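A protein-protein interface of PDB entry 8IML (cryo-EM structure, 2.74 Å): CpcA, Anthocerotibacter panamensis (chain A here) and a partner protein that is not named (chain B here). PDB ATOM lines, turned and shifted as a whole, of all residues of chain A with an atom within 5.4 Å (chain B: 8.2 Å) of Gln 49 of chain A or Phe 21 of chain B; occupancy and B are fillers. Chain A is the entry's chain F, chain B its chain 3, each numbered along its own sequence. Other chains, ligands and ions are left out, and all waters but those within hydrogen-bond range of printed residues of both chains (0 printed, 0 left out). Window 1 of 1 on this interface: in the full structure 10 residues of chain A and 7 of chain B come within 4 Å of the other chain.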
ATOM      1  N   ALA A  44     -18.503  -8.667  22.095  1.00  0.00           N
ATOM      2  CA  ALA A  44     -17.469  -9.228  21.236  1.00  0.00           C
ATOM      3  C   ALA A  44     -17.757 -10.681  20.890  1.00  0.00           C
ATOM      4  O   ALA A  44     -17.592 -11.092  19.737  1.00  0.00           O
ATOM      5  CB  ALA A  44     -16.108  -9.104  21.906  1.00  0.00           C
ATOM      6  N   LEU A  45     -18.187 -11.474  21.870  1.00  0.00           N
ATOM      7  CA  LEU A  45     -18.454 -12.883  21.604  1.00  0.00           C
ATOM      8  C   LEU A  45     -19.738 -13.078  20.812  1.00  0.00           C
ATOM      9  O   LEU A  45     -19.857 -14.056  20.070  1.00  0.00           O
ATOM     10  CB  LEU A  45     -18.511 -13.673  22.911  1.00  0.00           C
ATOM     11  CG  LEU A  45     -17.205 -14.254  23.456  1.00  0.00           C
ATOM     12  CD1 LEU A  45     -16.273 -13.174  23.917  1.00  0.00           C
ATOM     13  CD2 LEU A  45     -17.503 -15.201  24.588  1.00  0.00           C
ATOM     14  N   THR A  46     -20.706 -12.173  20.951  1.00  0.00           N
ATOM     15  CA  THR A  46     -21.909 -12.247  20.131  1.00  0.00           C
ATOM     16  C   THR A  46     -21.605 -11.895  18.684  1.00  0.00           C
ATOM     17  O   THR A  46     -22.109 -12.539  17.759  1.00  0.00           O
ATOM     18  CB  THR A  46     -22.970 -11.305  20.686  1.00  0.00           C
ATOM     19  OG1 THR A  46     -23.084 -11.482  22.103  1.00  0.00           O
ATOM     20  CG2 THR A  46     -24.299 -11.568  20.034  1.00  0.00           C
ATOM     21  N   LYS A  47     -20.782 -10.869  18.474  1.00  0.00           N
ATOM     22  CA  LYS A  47     -20.458 -10.425  17.126  1.00  0.00           C
ATOM     23  C   LYS A  47     -19.740 -11.511  16.342  1.00  0.00           C
ATOM     24  O   LYS A  47     -19.951 -11.660  15.135  1.00  0.00           O
ATOM     25  CB  LYS A  47     -19.604  -9.164  17.198  1.00  0.00           C
ATOM     26  CG  LYS A  47     -19.284  -8.544  15.857  1.00  0.00           C
ATOM     27  CD  LYS A  47     -19.543  -7.053  15.889  1.00  0.00           C
ATOM     28  CE  LYS A  47     -19.492  -6.447  14.499  1.00  0.00           C
ATOM     29  NZ  LYS A  47     -18.966  -5.057  14.539  1.00  0.00           N
ATOM     30  N   ASN A  48     -18.885 -12.276  17.010  1.00  0.00           N
ATOM     31  CA  ASN A  48     -18.036 -13.257  16.354  1.00  0.00           C
ATOM     32  C   ASN A  48     -18.509 -14.680  16.613  1.00  0.00           C
ATOM     33  O   ASN A  48     -17.717 -15.619  16.569  1.00  0.00           O
ATOM     34  CB  ASN A  48     -16.594 -13.080  16.815  1.00  0.00           C
ATOM     35  CG  ASN A  48     -16.029 -11.741  16.420  1.00  0.00           C
ATOM     36  OD1 ASN A  48     -15.725 -10.904  17.268  1.00  0.00           O
ATOM     37  ND2 ASN A  48     -15.892 -11.521  15.121  1.00  0.00           N
ATOM     38  N   GLN A  49     -19.807 -14.850  16.868  1.00  0.00           N
ATOM     39  CA  GLN A  49     -20.319 -16.137  17.324  1.00  0.00           C
ATOM     40  C   GLN A  49     -20.109 -17.219  16.278  1.00  0.00           C
ATOM     41  O   GLN A  49     -19.822 -18.372  16.614  1.00  0.00           O
ATOM     42  CB  GLN A  49     -21.804 -16.016  17.664  1.00  0.00           C
ATOM     43  CG  GLN A  49     -22.708 -16.220  16.469  1.00  0.00           C
ATOM     44  CD  GLN A  49     -24.113 -15.767  16.681  1.00  0.00           C
ATOM     45  OE1 GLN A  49     -24.424 -15.118  17.672  1.00  0.00           O
ATOM     46  NE2 GLN A  49     -24.985 -16.106  15.747  1.00  0.00           N
ATOM     47  N   ASP A  50     -20.218 -16.861  14.999  1.00  0.00           N
ATOM     48  CA  ASP A  50     -20.317 -17.878  13.962  1.00  0.00           C
ATOM     49  C   ASP A  50     -18.950 -18.452  13.630  1.00  0.00           C
ATOM     50  O   ASP A  50     -18.777 -19.674  13.569  1.00  0.00           O
ATOM     51  CB  ASP A  50     -20.973 -17.279  12.721  1.00  0.00           C
ATOM     52  CG  ASP A  50     -21.291 -18.320  11.677  1.00  0.00           C
ATOM     53  OD1 ASP A  50     -21.641 -19.450  12.066  1.00  0.00           O
ATOM     54  OD2 ASP A  50     -21.192 -18.009  10.471  1.00  0.00           O
ATOM     55  N   ALA A  51     -17.968 -17.577  13.418  1.00  0.00           N
ATOM     56  CA  ALA A  51     -16.604 -18.041  13.233  1.00  0.00           C
ATOM     57  C   ALA A  51     -16.128 -18.797  14.460  1.00  0.00           C
ATOM     58  O   ALA A  51     -15.467 -19.834  14.341  1.00  0.00           O
ATOM     59  CB  ALA A  51     -15.685 -16.859  12.936  1.00  0.00           C
ATOM     60  N   LEU A  52     -16.476 -18.302  15.650  1.00  0.00           N
ATOM     61  CA  LEU A  52     -16.125 -19.000  16.880  1.00  0.00           C
ATOM     62  C   LEU A  52     -16.652 -20.424  16.873  1.00  0.00           C
ATOM     63  O   LEU A  52     -15.898 -21.375  17.096  1.00  0.00           O
ATOM     64  CB  LEU A  52     -16.671 -18.243  18.087  1.00  0.00           C
ATOM     65  CG  LEU A  52     -15.783 -17.151  18.667  1.00  0.00           C
ATOM     66  CD1 LEU A  52     -16.501 -16.407  19.759  1.00  0.00           C
ATOM     67  CD2 LEU A  52     -14.532 -17.760  19.200  1.00  0.00           C
ATOM     68  N   VAL A  53     -17.945 -20.596  16.606  1.00  0.00           N
ATOM     69  CA  VAL A  53     -18.535 -21.920  16.745  1.00  0.00           C
ATOM     70  C   VAL A  53     -18.023 -22.858  15.660  1.00  0.00           C
ATOM     71  O   VAL A  53     -17.742 -24.032  15.925  1.00  0.00           O
ATOM     72  CB  VAL A  53     -20.069 -21.833  16.746  1.00  0.00           C
ATOM     73  CG1 VAL A  53     -20.660 -23.206  16.597  1.00  0.00           C
ATOM     74  CG2 VAL A  53     -20.553 -21.197  18.022  1.00  0.00           C
ATOM     75  N   LYS A  54     -17.881 -22.367  14.426  1.00  0.00           N
ATOM     76  CA  LYS A  54     -17.396 -23.245  13.366  1.00  0.00           C
ATOM     77  C   LYS A  54     -15.940 -23.637  13.588  1.00  0.00           C
ATOM     78  O   LYS A  54     -15.563 -24.801  13.383  1.00  0.00           O
ATOM     79  CB  LYS A  54     -17.604 -22.590  12.005  1.00  0.00           C
ATOM     80  CG  LYS A  54     -19.067 -22.301  11.706  1.00  0.00           C
ATOM     81  CD  LYS A  54     -19.295 -21.962  10.246  1.00  0.00           C
ATOM     82  CE  LYS A  54     -20.752 -21.593   9.989  1.00  0.00           C
ATOM     83  NZ  LYS A  54     -21.040 -21.276   8.561  1.00  0.00           N
ATOM     84  N   ALA A  84     -22.545 -28.404  16.223  1.00  0.00           N
ATOM     85  CA  ALA A  84     -22.508 -26.954  16.115  1.00  0.00           C
ATOM     86  C   ALA A  84     -23.589 -26.319  16.975  1.00  0.00           C
ATOM     87  O   ALA A  84     -23.358 -25.290  17.612  1.00  0.00           O
ATOM     88  CB  ALA A  84     -22.660 -26.533  14.657  1.00  0.00           C
ATOM     89  N   ARG A  85     -24.775 -26.923  17.007  1.00  0.00           N
ATOM     90  CA  ARG A  85     -25.854 -26.414  17.845  1.00  0.00           C
ATOM     91  C   ARG A  85     -25.478 -26.442  19.318  1.00  0.00           C
ATOM     92  O   ARG A  85     -25.778 -25.503  20.058  1.00  0.00           O
ATOM     93  CB  ARG A  85     -27.116 -27.231  17.598  1.00  0.00           C
ATOM     94  CG  ARG A  85     -28.281 -26.849  18.455  1.00  0.00           C
ATOM     95  CD  ARG A  85     -29.200 -28.020  18.633  1.00  0.00           C
ATOM     96  NE  ARG A  85     -28.521 -29.132  19.277  1.00  0.00           N
ATOM     97  CZ  ARG A  85     -29.119 -30.256  19.642  1.00  0.00           C
ATOM     98  NH1 ARG A  85     -30.412 -30.417  19.427  1.00  0.00           N
ATOM     99  NH2 ARG A  85     -28.427 -31.214  20.223  1.00  0.00           N
ATOM    100  N   GLY A  88     -22.913 -23.808  20.031  1.00  0.00           N
ATOM    101  CA  GLY A  88     -23.635 -22.551  20.030  1.00  0.00           C
ATOM    102  C   GLY A  88     -24.409 -22.332  21.312  1.00  0.00           C
ATOM    103  O   GLY A  88     -24.462 -21.218  21.828  1.00  0.00           O
ATOM    104  N   LEU A  91     -21.806 -21.324  24.009  1.00  0.00           N
ATOM    105  CA  LEU A  91     -21.375 -19.945  23.824  1.00  0.00           C
ATOM    106  C   LEU A  91     -22.479 -18.965  24.196  1.00  0.00           C
ATOM    107  O   LEU A  91     -22.222 -17.940  24.838  1.00  0.00           O
ATOM    108  CB  LEU A  91     -20.929 -19.744  22.382  1.00  0.00           C
ATOM    109  CG  LEU A  91     -20.380 -18.374  22.012  1.00  0.00           C
ATOM    110  CD1 LEU A  91     -19.085 -18.130  22.738  1.00  0.00           C
ATOM    111  CD2 LEU A  91     -20.186 -18.290  20.525  1.00  0.00           C
ATOM    112  N   GLU B  15     -29.058  -8.134  11.303  1.00  0.00           N
ATOM    113  CA  GLU B  15     -28.790  -8.190  12.734  1.00  0.00           C
ATOM    114  C   GLU B  15     -29.805  -9.058  13.466  1.00  0.00           C
ATOM    115  O   GLU B  15     -29.503  -9.578  14.544  1.00  0.00           O
ATOM    116  CB  GLU B  15     -28.729  -6.779  13.324  1.00  0.00           C
ATOM    117  CG  GLU B  15     -29.986  -5.956  13.224  1.00  0.00           C
ATOM    118  CD  GLU B  15     -30.891  -6.128  14.415  1.00  0.00           C
ATOM    119  OE1 GLU B  15     -30.396  -6.565  15.471  1.00  0.00           O
ATOM    120  OE2 GLU B  15     -32.096  -5.822  14.299  1.00  0.00           O
ATOM    121  N   LEU B  16     -30.998  -9.244  12.905  1.00  0.00           N
ATOM    122  CA  LEU B  16     -31.892 -10.261  13.443  1.00  0.00           C
ATOM    123  C   LEU B  16     -31.324 -11.652  13.223  1.00  0.00           C
ATOM    124  O   LEU B  16     -31.372 -12.497  14.122  1.00  0.00           O
ATOM    125  CB  LEU B  16     -33.275 -10.148  12.808  1.00  0.00           C
ATOM    126  CG  LEU B  16     -34.180  -9.031  13.327  1.00  0.00           C
ATOM    127  CD1 LEU B  16     -35.570  -9.166  12.748  1.00  0.00           C
ATOM    128  CD2 LEU B  16     -34.224  -9.028  14.836  1.00  0.00           C
ATOM    129  N   ALA B  17     -30.778 -11.910  12.036  1.00  0.00           N
ATOM    130  CA  ALA B  17     -30.216 -13.226  11.764  1.00  0.00           C
ATOM    131  C   ALA B  17     -28.852 -13.421  12.411  1.00  0.00           C
ATOM    132  O   ALA B  17     -28.396 -14.559  12.532  1.00  0.00           O
ATOM    133  CB  ALA B  17     -30.119 -13.454  10.259  1.00  0.00           C
ATOM    134  N   ALA B  18     -28.189 -12.341  12.814  1.00  0.00           N
ATOM    135  CA  ALA B  18     -26.890 -12.453  13.458  1.00  0.00           C
ATOM    136  C   ALA B  18     -27.006 -12.935  14.893  1.00  0.00           C
ATOM    137  O   ALA B  18     -26.043 -13.483  15.435  1.00  0.00           O
ATOM    138  CB  ALA B  18     -26.170 -11.108  13.424  1.00  0.00           C
ATOM    139  N   SER B  19     -28.164 -12.734  15.522  1.00  0.00           N
ATOM    140  CA  SER B  19     -28.344 -13.124  16.912  1.00  0.00           C
ATOM    141  C   SER B  19     -28.740 -14.583  17.055  1.00  0.00           C
ATOM    142  O   SER B  19     -28.851 -15.074  18.180  1.00  0.00           O
ATOM    143  CB  SER B  19     -29.392 -12.232  17.564  1.00  0.00           C
ATOM    144  OG  SER B  19     -30.672 -12.490  17.019  1.00  0.00           O
ATOM    145  N   ARG B  20     -28.963 -15.278  15.948  1.00  0.00           N
ATOM    146  CA  ARG B  20     -29.152 -16.717  15.919  1.00  0.00           C
ATOM    147  C   ARG B  20     -27.830 -17.355  15.547  1.00  0.00           C
ATOM    148  O   ARG B  20     -27.065 -16.782  14.767  1.00  0.00           O
ATOM    149  CB  ARG B  20     -30.173 -17.144  14.870  1.00  0.00           C
ATOM    150  CG  ARG B  20     -31.473 -16.385  14.782  1.00  0.00           C
ATOM    151  CD  ARG B  20     -32.015 -16.020  16.121  1.00  0.00           C
ATOM    152  NE  ARG B  20     -32.471 -17.203  16.843  1.00  0.00           N
ATOM    153  CZ  ARG B  20     -33.414 -18.045  16.428  1.00  0.00           C
ATOM    154  NH1 ARG B  20     -33.729 -19.088  17.179  1.00  0.00           N
ATOM    155  NH2 ARG B  20     -34.057 -17.846  15.286  1.00  0.00           N
ATOM    156  N   PHE B  21     -27.547 -18.534  16.076  1.00  0.00           N
ATOM    157  CA  PHE B  21     -26.523 -19.332  15.428  1.00  0.00           C
ATOM    158  C   PHE B  21     -27.131 -20.074  14.245  1.00  0.00           C
ATOM    159  O   PHE B  21     -28.082 -20.843  14.401  1.00  0.00           O
ATOM    160  CB  PHE B  21     -25.854 -20.316  16.379  1.00  0.00           C
ATOM    161  CG  PHE B  21     -24.943 -21.255  15.665  1.00  0.00           C
ATOM    162  CD1 PHE B  21     -23.721 -20.820  15.195  1.00  0.00           C
ATOM    163  CD2 PHE B  21     -25.327 -22.554  15.414  1.00  0.00           C
ATOM    164  CE1 PHE B  21     -22.902 -21.665  14.501  1.00  0.00           C
ATOM    165  CE2 PHE B  21     -24.505 -23.405  14.732  1.00  0.00           C
ATOM    166  CZ  PHE B  21     -23.289 -22.961  14.275  1.00  0.00           C
ATOM    167  N   GLY B  22     -26.570 -19.845  13.063  1.00  0.00           N
ATOM    168  CA  GLY B  22     -27.140 -20.386  11.853  1.00  0.00           C
ATOM    169  C   GLY B  22     -28.225 -19.539  11.238  1.00  0.00           C
ATOM    170  O   GLY B  22     -28.837 -19.965  10.253  1.00  0.00           O
ATOM    171  N   GLY B  23     -28.478 -18.353  11.775  1.00  0.00           N
ATOM    172  CA  GLY B  23     -29.532 -17.513  11.239  1.00  0.00           C
ATOM    173  C   GLY B  23     -30.878 -18.183  11.385  1.00  0.00           C
ATOM    174  O   GLY B  23     -31.265 -18.626  12.469  1.00  0.00           O
ATOM    175  N   PHE B  24     -31.608 -18.272  10.283  1.00  0.00           N
ATOM    176  CA  PHE B  24     -32.939 -18.865  10.284  1.00  0.00           C
ATOM    177  C   PHE B  24     -32.903 -20.154   9.477  1.00  0.00           C
ATOM    178  O   PHE B  24     -32.798 -20.123   8.247  1.00  0.00           O
ATOM    179  CB  PHE B  24     -33.970 -17.891   9.726  1.00  0.00           C
ATOM    180  CG  PHE B  24     -34.128 -16.648  10.542  1.00  0.00           C
ATOM    181  CD1 PHE B  24     -34.641 -16.707  11.821  1.00  0.00           C
ATOM    182  CD2 PHE B  24     -33.766 -15.421  10.033  1.00  0.00           C
ATOM    183  CE1 PHE B  24     -34.790 -15.570  12.571  1.00  0.00           C
ATOM    184  CE2 PHE B  24     -33.915 -14.279  10.783  1.00  0.00           C
ATOM    185  CZ  PHE B  24     -34.429 -14.355  12.053  1.00  0.00           C
ATOM    186  N   THR B  25     -32.979 -21.282  10.175  1.00  0.00           N
ATOM    187  CA  THR B  25     -33.098 -22.601   9.575  1.00  0.00           C
ATOM    188  C   THR B  25     -34.311 -23.295  10.175  1.00  0.00           C
ATOM    189  O   THR B  25     -34.870 -22.850  11.180  1.00  0.00           O
ATOM    190  CB  THR B  25     -31.838 -23.450   9.799  1.00  0.00           C
ATOM    191  OG1 THR B  25     -31.835 -23.953  11.135  1.00  0.00           O
ATOM    192  CG2 THR B  25     -30.587 -22.630   9.578  1.00  0.00           C
ATOM    193  N   GLU B  27     -34.186 -26.299  11.440  1.00  0.00           N
ATOM    194  CA  GLU B  27     -33.750 -27.129  12.555  1.00  0.00           C
ATOM    195  C   GLU B  27     -33.561 -26.340  13.846  1.00  0.00           C
ATOM    196  O   GLU B  27     -33.656 -26.920  14.932  1.00  0.00           O
ATOM    197  CB  GLU B  27     -32.451 -27.854  12.192  1.00  0.00           C
ATOM    198  CG  GLU B  27     -31.414 -26.965  11.531  1.00  0.00           C
ATOM    199  CD  GLU B  27     -30.165 -27.719  11.112  1.00  0.00           C
ATOM    200  OE1 GLU B  27     -29.174 -27.061  10.726  1.00  0.00           O
ATOM    201  OE2 GLU B  27     -30.174 -28.967  11.166  1.00  0.00           O
ATOM    202  N   ASN B  28     -33.299 -25.037  13.767  1.00  0.00           N
ATOM    203  CA  ASN B  28     -32.927 -24.247  14.936  1.00  0.00           C
ATOM    204  C   ASN B  28     -34.016 -23.264  15.360  1.00  0.00           C
ATOM    205  O   ASN B  28     -33.732 -22.145  15.780  1.00  0.00           O
ATOM    206  CB  ASN B  28     -31.609 -23.515  14.695  1.00  0.00           C
ATOM    207  CG  ASN B  28     -31.745 -22.349  13.738  1.00  0.00           C
ATOM    208  OD1 ASN B  28     -32.701 -22.263  12.974  1.00  0.00           O
ATOM    209  ND2 ASN B  28     -30.782 -21.439  13.782  1.00  0.00           N
ATOM    210  N   ILE B  29     -35.276 -23.678  15.287  1.00  0.00           N
ATOM    211  CA  ILE B  29     -36.385 -22.781  15.597  1.00  0.00           C
ATOM    212  C   ILE B  29     -36.693 -22.817  17.089  1.00  0.00           C
ATOM    213  O   ILE B  29     -36.382 -23.805  17.764  1.00  0.00           O
ATOM    214  CB  ILE B  29     -37.631 -23.146  14.780  1.00  0.00           C
ATOM    215  CG1 ILE B  29     -38.224 -24.450  15.290  1.00  0.00           C
ATOM    216  CG2 ILE B  29     -37.270 -23.296  13.322  1.00  0.00           C
ATOM    217  CD1 ILE B  29     -39.651 -24.657  14.893  1.00  0.00           C
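Hydrophobic or aromatic side chains of chain B within 4 Å of the printed part of chain A: Phe 21. Among the printed residues, 6 pairs touch across the chains.
ND2 of Asn 28 of chain B is in hydrogen-bond range of O of Phe 21 of chain B (2.8 Å). The backbone carbonyl oxygen (O) of Asn 28 of chain B sits at hydrogen-bond distance from the guanidinium group (NH1) of Arg 20 of chain B, at 3.4 Å. The side-chain carboxylate (OD2) of Asp 50 of chain A lies within salt-bridge range of the side-chain amino group (NZ) of Lys 54 of chain A (3.8 Å). OE1 of Gln 49 of chain A sits close to O of Thr 46 of chain A (3.5 Å).
The side-chain amide nitrogen (NE2) of Gln 49 of chain A sits at hydrogen-bond distance from the backbone carbonyl oxygen (O) of Ala 18 of chain B (2.8 Å). The side-chain amide nitrogen (NE2) of Gln 49 of chain A lies close to the backbone carbonyl oxygen (O) of Arg 20 of chain B, 2.4 Å away.
Ala 44 of chain A touches none of the printed residues of chain B. Of chain B, only Ala 18, Arg 20 and Phe 21 come within 4 Å of Gln 49 of chain A. Of the printed residues of chain A, Ala 18 of chain B touches Gln 49. Of the printed residues of chain A, Arg 20 of chain B touches Gln 49. Phe 21 of chain B touches just these residues of chain A: Gln 49, Asp 50, Val 53 and Ala 84. Thr 25 of chain B touches none of the printed residues of chain A. The nearest residue of chain B that does not touch Gln 49 of chain A is Ser 19 of chain B (4.3 Å).
Among the printed residues, merely in contact across the chains: Val 53 of chain A with Phe 21 of chain B (3.4 Å), Asp 50 of chain A with Phe 21 of chain B (3.5 Å), Gln 49 of chain A with Phe 21 of chain B (3.5 Å) and Ala 84 of chain A with Phe 21 of chain B (3.6 Å).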
